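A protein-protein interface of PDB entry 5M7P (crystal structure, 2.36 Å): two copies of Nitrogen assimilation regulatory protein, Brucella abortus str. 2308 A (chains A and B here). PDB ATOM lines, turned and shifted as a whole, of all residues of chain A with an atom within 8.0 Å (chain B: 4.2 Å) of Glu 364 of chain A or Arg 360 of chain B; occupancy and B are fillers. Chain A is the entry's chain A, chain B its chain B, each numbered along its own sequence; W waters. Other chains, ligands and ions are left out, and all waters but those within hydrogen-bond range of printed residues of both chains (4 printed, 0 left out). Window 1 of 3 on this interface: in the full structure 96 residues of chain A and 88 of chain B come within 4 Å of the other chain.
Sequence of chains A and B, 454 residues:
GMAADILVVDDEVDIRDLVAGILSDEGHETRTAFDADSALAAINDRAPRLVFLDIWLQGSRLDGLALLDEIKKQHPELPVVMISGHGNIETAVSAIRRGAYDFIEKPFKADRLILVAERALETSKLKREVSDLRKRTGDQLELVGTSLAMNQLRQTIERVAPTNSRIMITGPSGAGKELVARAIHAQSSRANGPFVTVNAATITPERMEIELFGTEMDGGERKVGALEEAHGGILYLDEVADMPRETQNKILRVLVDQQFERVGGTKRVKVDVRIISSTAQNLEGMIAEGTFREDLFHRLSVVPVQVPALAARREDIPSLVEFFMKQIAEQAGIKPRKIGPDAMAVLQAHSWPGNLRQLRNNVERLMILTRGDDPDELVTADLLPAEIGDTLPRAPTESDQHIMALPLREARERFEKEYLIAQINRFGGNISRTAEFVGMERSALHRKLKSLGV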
ATOM      1  N   VAL A 321     -12.705  10.115   2.823  1.00  0.00           N
ATOM      2  CA  VAL A 321     -13.599  10.995   2.056  1.00  0.00           C
ATOM      3  C   VAL A 321     -14.925  11.200   2.836  1.00  0.00           C
ATOM      4  O   VAL A 321     -15.363  12.338   2.987  1.00  0.00           O
ATOM      5  CB  VAL A 321     -13.809  10.523   0.576  1.00  0.00           C
ATOM      6  CG1 VAL A 321     -14.948  11.289  -0.116  1.00  0.00           C
ATOM      7  CG2 VAL A 321     -12.522  10.654  -0.231  1.00  0.00           C
ATOM      8  N   PHE A 324     -14.171  13.212   6.181  1.00  0.00           N
ATOM      9  CA  PHE A 324     -13.934  14.619   5.880  1.00  0.00           C
ATOM     10  C   PHE A 324     -15.224  15.337   5.477  1.00  0.00           C
ATOM     11  O   PHE A 324     -15.439  16.468   5.905  1.00  0.00           O
ATOM     12  CB  PHE A 324     -12.805  14.789   4.840  1.00  0.00           C
ATOM     13  CG  PHE A 324     -11.421  14.384   5.310  1.00  0.00           C
ATOM     14  CD1 PHE A 324     -10.978  14.704   6.593  1.00  0.00           C
ATOM     15  CD2 PHE A 324     -10.518  13.794   4.434  1.00  0.00           C
ATOM     16  CE1 PHE A 324      -9.682  14.363   7.011  1.00  0.00           C
ATOM     17  CE2 PHE A 324      -9.228  13.446   4.858  1.00  0.00           C
ATOM     18  CZ  PHE A 324      -8.821  13.730   6.141  1.00  0.00           C
ATOM     19  N   MET A 325     -16.119  14.648   4.735  1.00  0.00           N
ATOM     20  CA  MET A 325     -17.432  15.195   4.368  1.00  0.00           C
ATOM     21  C   MET A 325     -18.271  15.512   5.620  1.00  0.00           C
ATOM     22  O   MET A 325     -18.828  16.607   5.710  1.00  0.00           O
ATOM     23  CB  MET A 325     -18.214  14.253   3.456  1.00  0.00           C
ATOM     24  CG  MET A 325     -17.858  14.405   2.005  1.00  0.00           C
ATOM     25  SD  MET A 325     -19.155  13.832   0.880  1.00  0.00           S
ATOM     26  CE  MET A 325     -19.157  12.030   1.240  1.00  0.00           C
ATOM     27  N   ILE A 328     -16.764  18.631   7.432  1.00  0.00           N
ATOM     28  CA  ILE A 328     -17.047  19.871   6.712  1.00  0.00           C
ATOM     29  C   ILE A 328     -18.544  20.197   6.858  1.00  0.00           C
ATOM     30  O   ILE A 328     -18.910  21.370   6.947  1.00  0.00           O
ATOM     31  CB  ILE A 328     -16.536  19.773   5.234  1.00  0.00           C
ATOM     32  CG1 ILE A 328     -14.996  19.633   5.205  1.00  0.00           C
ATOM     33  CG2 ILE A 328     -16.976  20.968   4.382  1.00  0.00           C
ATOM     34  CD1 ILE A 328     -14.433  18.774   4.076  1.00  0.00           C
ATOM     35  N   GLN A 331     -18.860  21.801  10.200  1.00  0.00           N
ATOM     36  CA  GLN A 331     -18.253  23.133  10.156  1.00  0.00           C
ATOM     37  C   GLN A 331     -19.054  24.164   9.366  1.00  0.00           C
ATOM     38  O   GLN A 331     -19.360  25.241   9.888  1.00  0.00           O
ATOM     39  CB  GLN A 331     -16.853  23.059   9.532  1.00  0.00           C
ATOM     40  CG  GLN A 331     -15.762  22.570  10.450  1.00  0.00           C
ATOM     41  CD  GLN A 331     -14.497  22.428   9.659  1.00  0.00           C
ATOM     42  OE1 GLN A 331     -14.328  21.471   8.913  1.00  0.00           O
ATOM     43  NE2 GLN A 331     -13.619  23.413   9.749  1.00  0.00           N
ATOM     44  N   ALA A 332     -19.307  23.864   8.077  1.00  0.00           N
ATOM     45  CA  ALA A 332     -19.934  24.743   7.095  1.00  0.00           C
ATOM     46  C   ALA A 332     -21.443  24.684   7.008  1.00  0.00           C
ATOM     47  O   ALA A 332     -22.036  25.607   6.460  1.00  0.00           O
ATOM     48  CB  ALA A 332     -19.349  24.455   5.723  1.00  0.00           C
ATOM     49  N   ILE A 334     -22.944  22.257   5.181  1.00  0.00           N
ATOM     50  CA  ILE A 334     -23.214  21.761   3.829  1.00  0.00           C
ATOM     51  C   ILE A 334     -23.636  20.286   3.980  1.00  0.00           C
ATOM     52  O   ILE A 334     -22.930  19.511   4.628  1.00  0.00           O
ATOM     53  CB  ILE A 334     -21.993  21.955   2.858  1.00  0.00           C
ATOM     54  CG1 ILE A 334     -21.572  23.443   2.747  1.00  0.00           C
ATOM     55  CG2 ILE A 334     -22.246  21.329   1.461  1.00  0.00           C
ATOM     56  CD1 ILE A 334     -20.233  23.710   1.968  1.00  0.00           C
ATOM     57  N   ARG A 357      -3.959  16.109   4.302  1.00  0.00           N
ATOM     58  CA  ARG A 357      -4.321  17.533   4.231  1.00  0.00           C
ATOM     59  C   ARG A 357      -4.858  17.853   2.821  1.00  0.00           C
ATOM     60  O   ARG A 357      -5.925  18.458   2.680  1.00  0.00           O
ATOM     61  CB  ARG A 357      -3.129  18.451   4.554  1.00  0.00           C
ATOM     62  CG  ARG A 357      -3.600  19.909   4.722  1.00  0.00           C
ATOM     63  CD  ARG A 357      -2.555  20.910   5.169  1.00  0.00           C
ATOM     64  NE  ARG A 357      -1.364  20.242   5.664  1.00  0.00           N
ATOM     65  CZ  ARG A 357      -1.197  19.807   6.904  1.00  0.00           C
ATOM     66  NH1 ARG A 357      -2.139  20.023   7.826  1.00  0.00           N
ATOM     67  NH2 ARG A 357      -0.093  19.165   7.240  1.00  0.00           N
ATOM     68  N   GLN A 358      -4.107  17.427   1.782  1.00  0.00           N
ATOM     69  CA  GLN A 358      -4.497  17.628   0.398  1.00  0.00           C
ATOM     70  C   GLN A 358      -5.847  16.952   0.102  1.00  0.00           C
ATOM     71  O   GLN A 358      -6.707  17.585  -0.496  1.00  0.00           O
ATOM     72  CB  GLN A 358      -3.403  17.132  -0.530  1.00  0.00           C
ATOM     73  CG  GLN A 358      -3.479  17.756  -1.903  1.00  0.00           C
ATOM     74  CD  GLN A 358      -2.577  17.084  -2.901  1.00  0.00           C
ATOM     75  OE1 GLN A 358      -1.874  16.125  -2.609  1.00  0.00           O
ATOM     76  NE2 GLN A 358      -2.578  17.585  -4.106  1.00  0.00           N
ATOM     77  N   LEU A 359      -6.051  15.702   0.559  1.00  0.00           N
ATOM     78  CA  LEU A 359      -7.339  15.019   0.371  1.00  0.00           C
ATOM     79  C   LEU A 359      -8.496  15.821   0.988  1.00  0.00           C
ATOM     80  O   LEU A 359      -9.509  16.050   0.307  1.00  0.00           O
ATOM     81  CB  LEU A 359      -7.324  13.575   0.921  1.00  0.00           C
ATOM     82  CG  LEU A 359      -8.663  12.793   0.867  1.00  0.00           C
ATOM     83  CD1 LEU A 359      -9.216  12.697  -0.558  1.00  0.00           C
ATOM     84  CD2 LEU A 359      -8.496  11.405   1.434  1.00  0.00           C
ATOM     85  N   ARG A 360      -8.326  16.273   2.260  1.00  0.00           N
ATOM     86  CA  ARG A 360      -9.336  17.038   3.004  1.00  0.00           C
ATOM     87  C   ARG A 360      -9.686  18.337   2.286  1.00  0.00           C
ATOM     88  O   ARG A 360     -10.873  18.646   2.129  1.00  0.00           O
ATOM     89  CB  ARG A 360      -8.858  17.330   4.434  1.00  0.00           C
ATOM     90  CG  ARG A 360      -9.947  17.926   5.319  1.00  0.00           C
ATOM     91  CD  ARG A 360      -9.342  18.731   6.434  1.00  0.00           C
ATOM     92  NE  ARG A 360     -10.355  19.192   7.374  1.00  0.00           N
ATOM     93  CZ  ARG A 360     -11.014  20.343   7.277  1.00  0.00           C
ATOM     94  NH1 ARG A 360     -10.788  21.165   6.256  1.00  0.00           N
ATOM     95  NH2 ARG A 360     -11.903  20.681   8.196  1.00  0.00           N
ATOM     96  N   ASN A 361      -8.655  19.084   1.848  1.00  0.00           N
ATOM     97  CA  ASN A 361      -8.805  20.338   1.123  1.00  0.00           C
ATOM     98  C   ASN A 361      -9.563  20.131  -0.231  1.00  0.00           C
ATOM     99  O   ASN A 361     -10.317  21.014  -0.665  1.00  0.00           O
ATOM    100  CB  ASN A 361      -7.422  21.000   0.940  1.00  0.00           C
ATOM    101  CG  ASN A 361      -7.435  22.176  -0.007  1.00  0.00           C
ATOM    102  OD1 ASN A 361      -7.102  22.053  -1.181  1.00  0.00           O
ATOM    103  ND2 ASN A 361      -7.855  23.331   0.466  1.00  0.00           N
ATOM    104  N   ASN A 362      -9.405  18.949  -0.855  1.00  0.00           N
ATOM    105  CA  ASN A 362     -10.097  18.659  -2.101  1.00  0.00           C
ATOM    106  C   ASN A 362     -11.557  18.273  -1.856  1.00  0.00           C
ATOM    107  O   ASN A 362     -12.425  18.648  -2.654  1.00  0.00           O
ATOM    108  CB  ASN A 362      -9.328  17.639  -2.960  1.00  0.00           C
ATOM    109  CG  ASN A 362      -8.231  18.328  -3.726  1.00  0.00           C
ATOM    110  OD1 ASN A 362      -8.488  19.042  -4.693  1.00  0.00           O
ATOM    111  ND2 ASN A 362      -7.020  18.307  -3.199  1.00  0.00           N
ATOM    112  N   VAL A 363     -11.839  17.587  -0.741  1.00  0.00           N
ATOM    113  CA  VAL A 363     -13.212  17.214  -0.343  1.00  0.00           C
ATOM    114  C   VAL A 363     -13.999  18.491  -0.008  1.00  0.00           C
ATOM    115  O   VAL A 363     -15.115  18.674  -0.512  1.00  0.00           O
ATOM    116  CB  VAL A 363     -13.225  16.152   0.781  1.00  0.00           C
ATOM    117  CG1 VAL A 363     -14.633  15.916   1.311  1.00  0.00           C
ATOM    118  CG2 VAL A 363     -12.608  14.834   0.297  1.00  0.00           C
ATOM    119  N   GLU A 364     -13.379  19.417   0.745  1.00  0.00           N
ATOM    120  CA  GLU A 364     -13.972  20.718   1.080  1.00  0.00           C
ATOM    121  C   GLU A 364     -14.290  21.477  -0.219  1.00  0.00           C
ATOM    122  O   GLU A 364     -15.404  21.952  -0.392  1.00  0.00           O
ATOM    123  CB  GLU A 364     -13.037  21.531   1.996  1.00  0.00           C
ATOM    124  CG  GLU A 364     -13.688  22.795   2.544  1.00  0.00           C
ATOM    125  CD  GLU A 364     -12.792  23.769   3.296  1.00  0.00           C
ATOM    126  OE1 GLU A 364     -11.619  23.949   2.894  1.00  0.00           O
ATOM    127  OE2 GLU A 364     -13.291  24.407   4.250  1.00  0.00           O
ATOM    128  N   ARG A 365     -13.321  21.534  -1.148  1.00  0.00           N
ATOM    129  CA  ARG A 365     -13.467  22.157  -2.466  1.00  0.00           C
ATOM    130  C   ARG A 365     -14.738  21.636  -3.191  1.00  0.00           C
ATOM    131  O   ARG A 365     -15.524  22.432  -3.695  1.00  0.00           O
ATOM    132  CB  ARG A 365     -12.207  21.869  -3.302  1.00  0.00           C
ATOM    133  CG  ARG A 365     -12.247  22.501  -4.677  1.00  0.00           C
ATOM    134  CD  ARG A 365     -11.244  21.865  -5.628  1.00  0.00           C
ATOM    135  NE  ARG A 365     -11.691  21.987  -7.014  1.00  0.00           N
ATOM    136  CZ  ARG A 365     -11.622  23.112  -7.713  1.00  0.00           C
ATOM    137  NH1 ARG A 365     -11.095  24.203  -7.175  1.00  0.00           N
ATOM    138  NH2 ARG A 365     -12.082  23.154  -8.957  1.00  0.00           N
ATOM    139  N   LEU A 366     -14.936  20.308  -3.199  1.00  0.00           N
ATOM    140  CA  LEU A 366     -16.071  19.614  -3.810  1.00  0.00           C
ATOM    141  C   LEU A 366     -17.401  19.966  -3.147  1.00  0.00           C
ATOM    142  O   LEU A 366     -18.414  20.100  -3.828  1.00  0.00           O
ATOM    143  CB  LEU A 366     -15.850  18.084  -3.773  1.00  0.00           C
ATOM    144  CG  LEU A 366     -14.707  17.524  -4.650  1.00  0.00           C
ATOM    145  CD1 LEU A 366     -14.598  16.021  -4.497  1.00  0.00           C
ATOM    146  CD2 LEU A 366     -14.875  17.917  -6.140  1.00  0.00           C
ATOM    147  N   MET A 367     -17.391  20.122  -1.825  1.00  0.00           N
ATOM    148  CA  MET A 367     -18.578  20.481  -1.066  1.00  0.00           C
ATOM    149  C   MET A 367     -18.934  21.936  -1.225  1.00  0.00           C
ATOM    150  O   MET A 367     -20.117  22.260  -1.316  1.00  0.00           O
ATOM    151  CB  MET A 367     -18.413  20.070   0.379  1.00  0.00           C
ATOM    152  CG  MET A 367     -18.488  18.570   0.535  1.00  0.00           C
ATOM    153  SD  MET A 367     -18.024  18.114   2.201  1.00  0.00           S
ATOM    154  CE  MET A 367     -19.646  18.370   3.067  1.00  0.00           C
ATOM    155  N   ILE A 368     -17.916  22.816  -1.326  1.00  0.00           N
ATOM    156  CA  ILE A 368     -18.125  24.248  -1.550  1.00  0.00           C
ATOM    157  C   ILE A 368     -18.771  24.439  -2.930  1.00  0.00           C
ATOM    158  O   ILE A 368     -19.835  25.047  -3.012  1.00  0.00           O
ATOM    159  CB  ILE A 368     -16.806  25.063  -1.412  1.00  0.00           C
ATOM    160  CG1 ILE A 368     -16.304  25.081   0.042  1.00  0.00           C
ATOM    161  CG2 ILE A 368     -16.966  26.506  -1.966  1.00  0.00           C
ATOM    162  CD1 ILE A 368     -14.858  25.657   0.205  1.00  0.00           C
ATOM    163  N   LEU A 369     -18.150  23.870  -3.995  1.00  0.00           N
ATOM    164  CA  LEU A 369     -18.616  23.984  -5.375  1.00  0.00           C
ATOM    165  C   LEU A 369     -19.955  23.328  -5.670  1.00  0.00           C
ATOM    166  O   LEU A 369     -20.574  23.713  -6.657  1.00  0.00           O
ATOM    167  CB  LEU A 369     -17.555  23.468  -6.371  1.00  0.00           C
ATOM    168  CG  LEU A 369     -16.267  24.276  -6.443  1.00  0.00           C
ATOM    169  CD1 LEU A 369     -15.200  23.492  -7.111  1.00  0.00           C
ATOM    170  CD2 LEU A 369     -16.480  25.600  -7.152  1.00  0.00           C
ATOM    171  N   THR A 370     -20.400  22.341  -4.875  1.00  0.00           N
ATOM    172  CA  THR A 370     -21.696  21.706  -5.134  1.00  0.00           C
ATOM    173  C   THR A 370     -22.786  22.166  -4.155  1.00  0.00           C
ATOM    174  O   THR A 370     -23.880  21.591  -4.139  1.00  0.00           O
ATOM    175  CB  THR A 370     -21.596  20.181  -5.208  1.00  0.00           C
ATOM    176  OG1 THR A 370     -21.072  19.684  -3.987  1.00  0.00           O
ATOM    177  CG2 THR A 370     -20.790  19.691  -6.403  1.00  0.00           C
ATOM    178  N   ARG A 371     -22.490  23.190  -3.336  1.00  0.00           N
ATOM    179  CA  ARG A 371     -23.449  23.744  -2.376  1.00  0.00           C
ATOM    180  C   ARG A 371     -24.583  24.401  -3.168  1.00  0.00           C
ATOM    181  O   ARG A 371     -24.326  25.200  -4.073  1.00  0.00           O
ATOM    182  CB  ARG A 371     -22.759  24.752  -1.425  1.00  0.00           C
ATOM    183  CG  ARG A 371     -23.713  25.530  -0.521  1.00  0.00           C
ATOM    184  CD  ARG A 371     -22.990  26.251   0.582  1.00  0.00           C
ATOM    185  NE  ARG A 371     -23.724  26.127   1.840  1.00  0.00           N
ATOM    186  CZ  ARG A 371     -23.255  26.474   3.033  1.00  0.00           C
ATOM    187  NH1 ARG A 371     -22.027  26.966   3.155  1.00  0.00           N
ATOM    188  NH2 ARG A 371     -24.001  26.312   4.115  1.00  0.00           N
ATOM    189  N   PHE B 324      -5.442  34.222   6.364  1.00  0.00           N
ATOM    190  CA  PHE B 324      -5.609  32.783   6.164  1.00  0.00           C
ATOM    191  C   PHE B 324      -4.270  32.042   6.033  1.00  0.00           C
ATOM    192  O   PHE B 324      -4.162  30.915   6.516  1.00  0.00           O
ATOM    193  CB  PHE B 324      -6.553  32.475   4.984  1.00  0.00           C
ATOM    194  CG  PHE B 324      -7.998  32.883   5.179  1.00  0.00           C
ATOM    195  CD1 PHE B 324      -8.651  32.651   6.392  1.00  0.00           C
ATOM    196  CD2 PHE B 324      -8.726  33.448   4.132  1.00  0.00           C
ATOM    197  CE1 PHE B 324      -9.999  32.986   6.553  1.00  0.00           C
ATOM    198  CE2 PHE B 324     -10.069  33.799   4.298  1.00  0.00           C
ATOM    199  CZ  PHE B 324     -10.691  33.582   5.513  1.00  0.00           C
ATOM    200  N   LEU B 356     -15.797  33.727   1.751  1.00  0.00           N
ATOM    201  CA  LEU B 356     -14.600  33.546   2.594  1.00  0.00           C
ATOM    202  C   LEU B 356     -14.225  32.109   2.820  1.00  0.00           C
ATOM    203  O   LEU B 356     -13.025  31.807   2.892  1.00  0.00           O
ATOM    204  CB  LEU B 356     -14.709  34.299   3.924  1.00  0.00           C
ATOM    205  CG  LEU B 356     -14.464  35.820   3.808  1.00  0.00           C
ATOM    206  CD1 LEU B 356     -15.654  36.547   3.149  1.00  0.00           C
ATOM    207  CD2 LEU B 356     -14.106  36.420   5.133  1.00  0.00           C
ATOM    208  N   ARG B 357     -15.217  31.212   2.920  1.00  0.00           N
ATOM    209  CA  ARG B 357     -14.935  29.781   3.042  1.00  0.00           C
ATOM    210  C   ARG B 357     -14.222  29.304   1.758  1.00  0.00           C
ATOM    211  O   ARG B 357     -13.265  28.550   1.847  1.00  0.00           O
ATOM    212  CB  ARG B 357     -16.223  28.990   3.264  1.00  0.00           C
ATOM    213  CG  ARG B 357     -16.013  27.491   3.194  1.00  0.00           C
ATOM    214  CD  ARG B 357     -17.106  26.735   3.861  1.00  0.00           C
ATOM    215  NE  ARG B 357     -17.083  26.964   5.297  1.00  0.00           N
ATOM    216  CZ  ARG B 357     -18.007  27.645   5.959  1.00  0.00           C
ATOM    217  NH1 ARG B 357     -17.922  27.776   7.274  1.00  0.00           N
ATOM    218  NH2 ARG B 357     -19.042  28.179   5.313  1.00  0.00           N
ATOM    219  N   GLN B 358     -14.685  29.764   0.583  1.00  0.00           N
ATOM    220  CA  GLN B 358     -14.076  29.452  -0.715  1.00  0.00           C
ATOM    221  C   GLN B 358     -12.661  30.087  -0.858  1.00  0.00           C
ATOM    222  O   GLN B 358     -11.754  29.432  -1.377  1.00  0.00           O
ATOM    223  CB  GLN B 358     -14.994  29.895  -1.855  1.00  0.00           C
ATOM    224  CG  GLN B 358     -14.576  29.329  -3.198  1.00  0.00           C
ATOM    225  CD  GLN B 358     -15.463  29.801  -4.311  1.00  0.00           C
ATOM    226  OE1 GLN B 358     -16.265  30.744  -4.150  1.00  0.00           O
ATOM    227  NE2 GLN B 358     -15.301  29.169  -5.475  1.00  0.00           N
ATOM    228  N   LEU B 359     -12.484  31.348  -0.398  1.00  0.00           N
ATOM    229  CA  LEU B 359     -11.188  32.044  -0.410  1.00  0.00           C
ATOM    230  C   LEU B 359     -10.141  31.274   0.415  1.00  0.00           C
ATOM    231  O   LEU B 359      -9.051  30.985  -0.098  1.00  0.00           O
ATOM    232  CB  LEU B 359     -11.327  33.508   0.093  1.00  0.00           C
ATOM    233  CG  LEU B 359     -10.051  34.382   0.122  1.00  0.00           C
ATOM    234  CD1 LEU B 359      -9.455  34.574  -1.287  1.00  0.00           C
ATOM    235  CD2 LEU B 359     -10.340  35.744   0.733  1.00  0.00           C
ATOM    236  N   ARG B 360     -10.492  30.907   1.670  1.00  0.00           N
ATOM    237  CA  ARG B 360      -9.621  30.158   2.583  1.00  0.00           C
ATOM    238  C   ARG B 360      -9.212  28.807   1.944  1.00  0.00           C
ATOM    239  O   ARG B 360      -8.020  28.474   1.892  1.00  0.00           O
ATOM    240  CB  ARG B 360     -10.347  29.942   3.927  1.00  0.00           C
ATOM    241  CG  ARG B 360      -9.439  29.598   5.108  1.00  0.00           C
ATOM    242  CD  ARG B 360     -10.073  28.613   6.076  1.00  0.00           C
ATOM    243  NE  ARG B 360      -9.655  27.265   5.685  1.00  0.00           N
ATOM    244  CZ  ARG B 360     -10.356  26.441   4.911  1.00  0.00           C
ATOM    245  NH1 ARG B 360     -11.584  26.770   4.511  1.00  0.00           N
ATOM    246  NH2 ARG B 360      -9.848  25.269   4.554  1.00  0.00           N
ATOM    247  N   ASN B 361     -10.193  28.083   1.389  1.00  0.00           N
ATOM    248  CA  ASN B 361      -9.973  26.790   0.738  1.00  0.00           C
ATOM    249  C   ASN B 361      -8.952  26.906  -0.412  1.00  0.00           C
ATOM    250  O   ASN B 361      -8.062  26.069  -0.510  1.00  0.00           O
ATOM    251  CB  ASN B 361     -11.306  26.205   0.261  1.00  0.00           C
ATOM    252  CG  ASN B 361     -11.176  24.944  -0.573  1.00  0.00           C
ATOM    253  OD1 ASN B 361     -11.247  24.986  -1.806  1.00  0.00           O
ATOM    254  ND2 ASN B 361     -11.034  23.792   0.079  1.00  0.00           N
ATOM    255  N   ASN B 362      -9.054  27.983  -1.223  1.00  0.00           N
ATOM    256  CA  ASN B 362      -8.154  28.283  -2.330  1.00  0.00           C
ATOM    257  C   ASN B 362      -6.769  28.664  -1.874  1.00  0.00           C
ATOM    258  O   ASN B 362      -5.799  28.217  -2.478  1.00  0.00           O
ATOM    259  CB  ASN B 362      -8.754  29.336  -3.256  1.00  0.00           C
ATOM    260  CG  ASN B 362      -9.585  28.681  -4.313  1.00  0.00           C
ATOM    261  OD1 ASN B 362      -9.049  28.119  -5.269  1.00  0.00           O
ATOM    262  ND2 ASN B 362     -10.900  28.664  -4.132  1.00  0.00           N
ATOM    263  N   VAL B 363      -6.668  29.441  -0.787  1.00  0.00           N
ATOM    264  CA  VAL B 363      -5.392  29.849  -0.157  1.00  0.00           C
ATOM    265  C   VAL B 363      -4.676  28.589   0.354  1.00  0.00           C
ATOM    266  O   VAL B 363      -3.492  28.416   0.109  1.00  0.00           O
ATOM    267  CB  VAL B 363      -5.625  30.888   0.986  1.00  0.00           C
ATOM    268  CG1 VAL B 363      -4.343  31.156   1.754  1.00  0.00           C
ATOM    269  CG2 VAL B 363      -6.196  32.202   0.444  1.00  0.00           C
ATOM    270  N   GLU B 364      -5.408  27.697   1.021  1.00  0.00           N
ATOM    271  CA  GLU B 364      -4.858  26.455   1.562  1.00  0.00           C
ATOM    272  C   GLU B 364      -4.341  25.531   0.448  1.00  0.00           C
ATOM    273  O   GLU B 364      -3.253  24.962   0.590  1.00  0.00           O
ATOM    274  CB  GLU B 364      -5.893  25.744   2.436  1.00  0.00           C
ATOM    275  CG  GLU B 364      -5.332  24.520   3.135  1.00  0.00           C
ATOM    276  CD  GLU B 364      -6.347  23.582   3.748  1.00  0.00           C
ATOM    277  OE1 GLU B 364      -7.514  23.572   3.290  1.00  0.00           O
ATOM    278  OE2 GLU B 364      -5.961  22.828   4.669  1.00  0.00           O
HETATM  279  O   HOH W   1      -7.002  20.371   4.701  1.00  0.00           O
HETATM  280  O   HOH W   2      -9.653  21.987   3.850  1.00  0.00           O
HETATM  281  O   HOH W   3      -9.524  24.711  -4.163  1.00  0.00           O
HETATM  282  O   HOH W   4     -11.589  24.098   6.891  1.00  0.00           O
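O of Asn 361 of chain B lies within hydrogen-bond range of ND2 of Asn 361 of chain A (2.9 Å). The backbone NH (N) of Arg 365 of chain A sits close to the side-chain amide nitrogen (ND2) of Asn 361 of chain B. The side-chain carboxylate (OE1) of Glu 364 of chain B lies within hydrogen-bond range of the side-chain amide nitrogen (ND2) of Asn 361 of chain A, 2.9 Å away. The guanidinium group of Arg 360 of chain B is in salt-bridge range of the side-chain carboxylate of Glu 364 of chain A (2.8 Å). The side-chain carboxylate of Glu 364 of chain A lies within hydrogen-bond range of the side-chain amide nitrogen of Asn 361 of chain B, 2.9 Å away.
The side-chain amide oxygen of Gln 331 of chain A sits at hydrogen-bond distance from the guanidinium group of Arg 360 of chain A, 2.6 Å away. The side-chain carboxylate (OE1) of Glu 364 of chain B lies within salt-bridge range of the guanidinium group (NH2) of Arg 360 of chain B. O of Ala 332 of chain A lies within hydrogen-bond range of NH2 of Arg 371 of chain A, at 3.1 Å. O of Gln 358 of chain B sits at hydrogen-bond distance from ND2 of Asn 362 of chain B (3.0 Å).
Among the printed residues, pairs that only touch across the chains: Ala 332 of chain A with Arg 357 of chain B (3.4 Å), Ile 368 of chain A with Asn 361 of chain B (3.6 Å), Ile 368 of chain A with Arg 357 of chain B (3.7 Å), Arg 357 of chain A with Glu 364 of chain B (3.8 Å), Arg 371 of chain A with Arg 357 of chain B (3.9 Å), Ile 368 of chain A with Gln 358 of chain B (3.9 Å) and Gln 331 of chain A with Arg 357 of chain B (3.9 Å).
Of the printed residues of chain B, Gln 331 of chain A touches Arg 357 (3.9 Å). Ile 334 of chain A touches none of the printed residues of chain B. Glu 364 of chain A touches just these residues of chain B: Arg 360 (2.8 Å) and Asn 361 (2.9 Å). Leu 366 of chain A touches none of the printed residues of chain B. Of the printed residues of chain B, Ile 368 of chain A touches Arg 357, Gln 358 and Asn 361. Arg 360 of chain B touches one residue of chain A. Printed residues of chain A within 4 Å of Glu 364 of chain B: Arg 357 and Asn 361. The nearest residue of chain A that does not touch Arg 360 of chain B is Arg 360 of chain A (4.5 Å).
Hydrophobic or aromatic side chains of chain A within 4 Å of the printed part of chain B: Ala 332 and Ile 368. Printed residues of chain B that touch a printed residue of chain A: Arg 357, Gln 358, Arg 360, Asn 361 and Glu 364. Along chain B the printed residues that touch a printed residue of chain A span positions 357 to 364. Among the printed residues, 12 pairs touch across the chains.
Arg 357 of chain A touches Glu 364 of chain B, but with the chains exchanged Glu 364 of chain A does not touch Arg 357 of chain B (4.2 Å). Asn 361 of chain B touches its own counterpart, Asn 361 of chain A. Asn 361 of chain A touches Glu 364 of chain B, and with the chains exchanged Glu 364 of chain A touches Asn 361 of chain B. Glu 364 of chain A touches Arg 360 of chain B, but with the chains exchanged Arg 360 of chain A does not touch Glu 364 of chain B (5.0 Å). 9 positions are printed for both chains. Of the 12 pairs that touch across the chains among the printed residues, 3 have their exchanged pair printed and touching as well.
Water W1 lies within hydrogen-bond range of the side-chain carboxylate of Glu 364 of chain B (2.7 Å) and the backbone carbonyl oxygen of Arg 357 of chain A (3.0 Å). Water W2 lies within hydrogen-bond range of OE1 of Glu 364 of chain B (2.7 Å), NH1 of Arg 360 of chain A (2.8 Å), OE1 of Glu 364 of chain A (2.9 Å) and NH2 of Arg 360 of chain B (3.4 Å). Water W3 bridges OD1 of Asn 361 of chain B and NH1 of Arg 365 of chain A. Water W4 lies within hydrogen-bond range of NH1 of Arg 360 of chain A (3.1 Å), NH2 of Arg 360 of chain B (3.1 Å) and OE2 of Glu 364 of chain A (3.2 Å).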
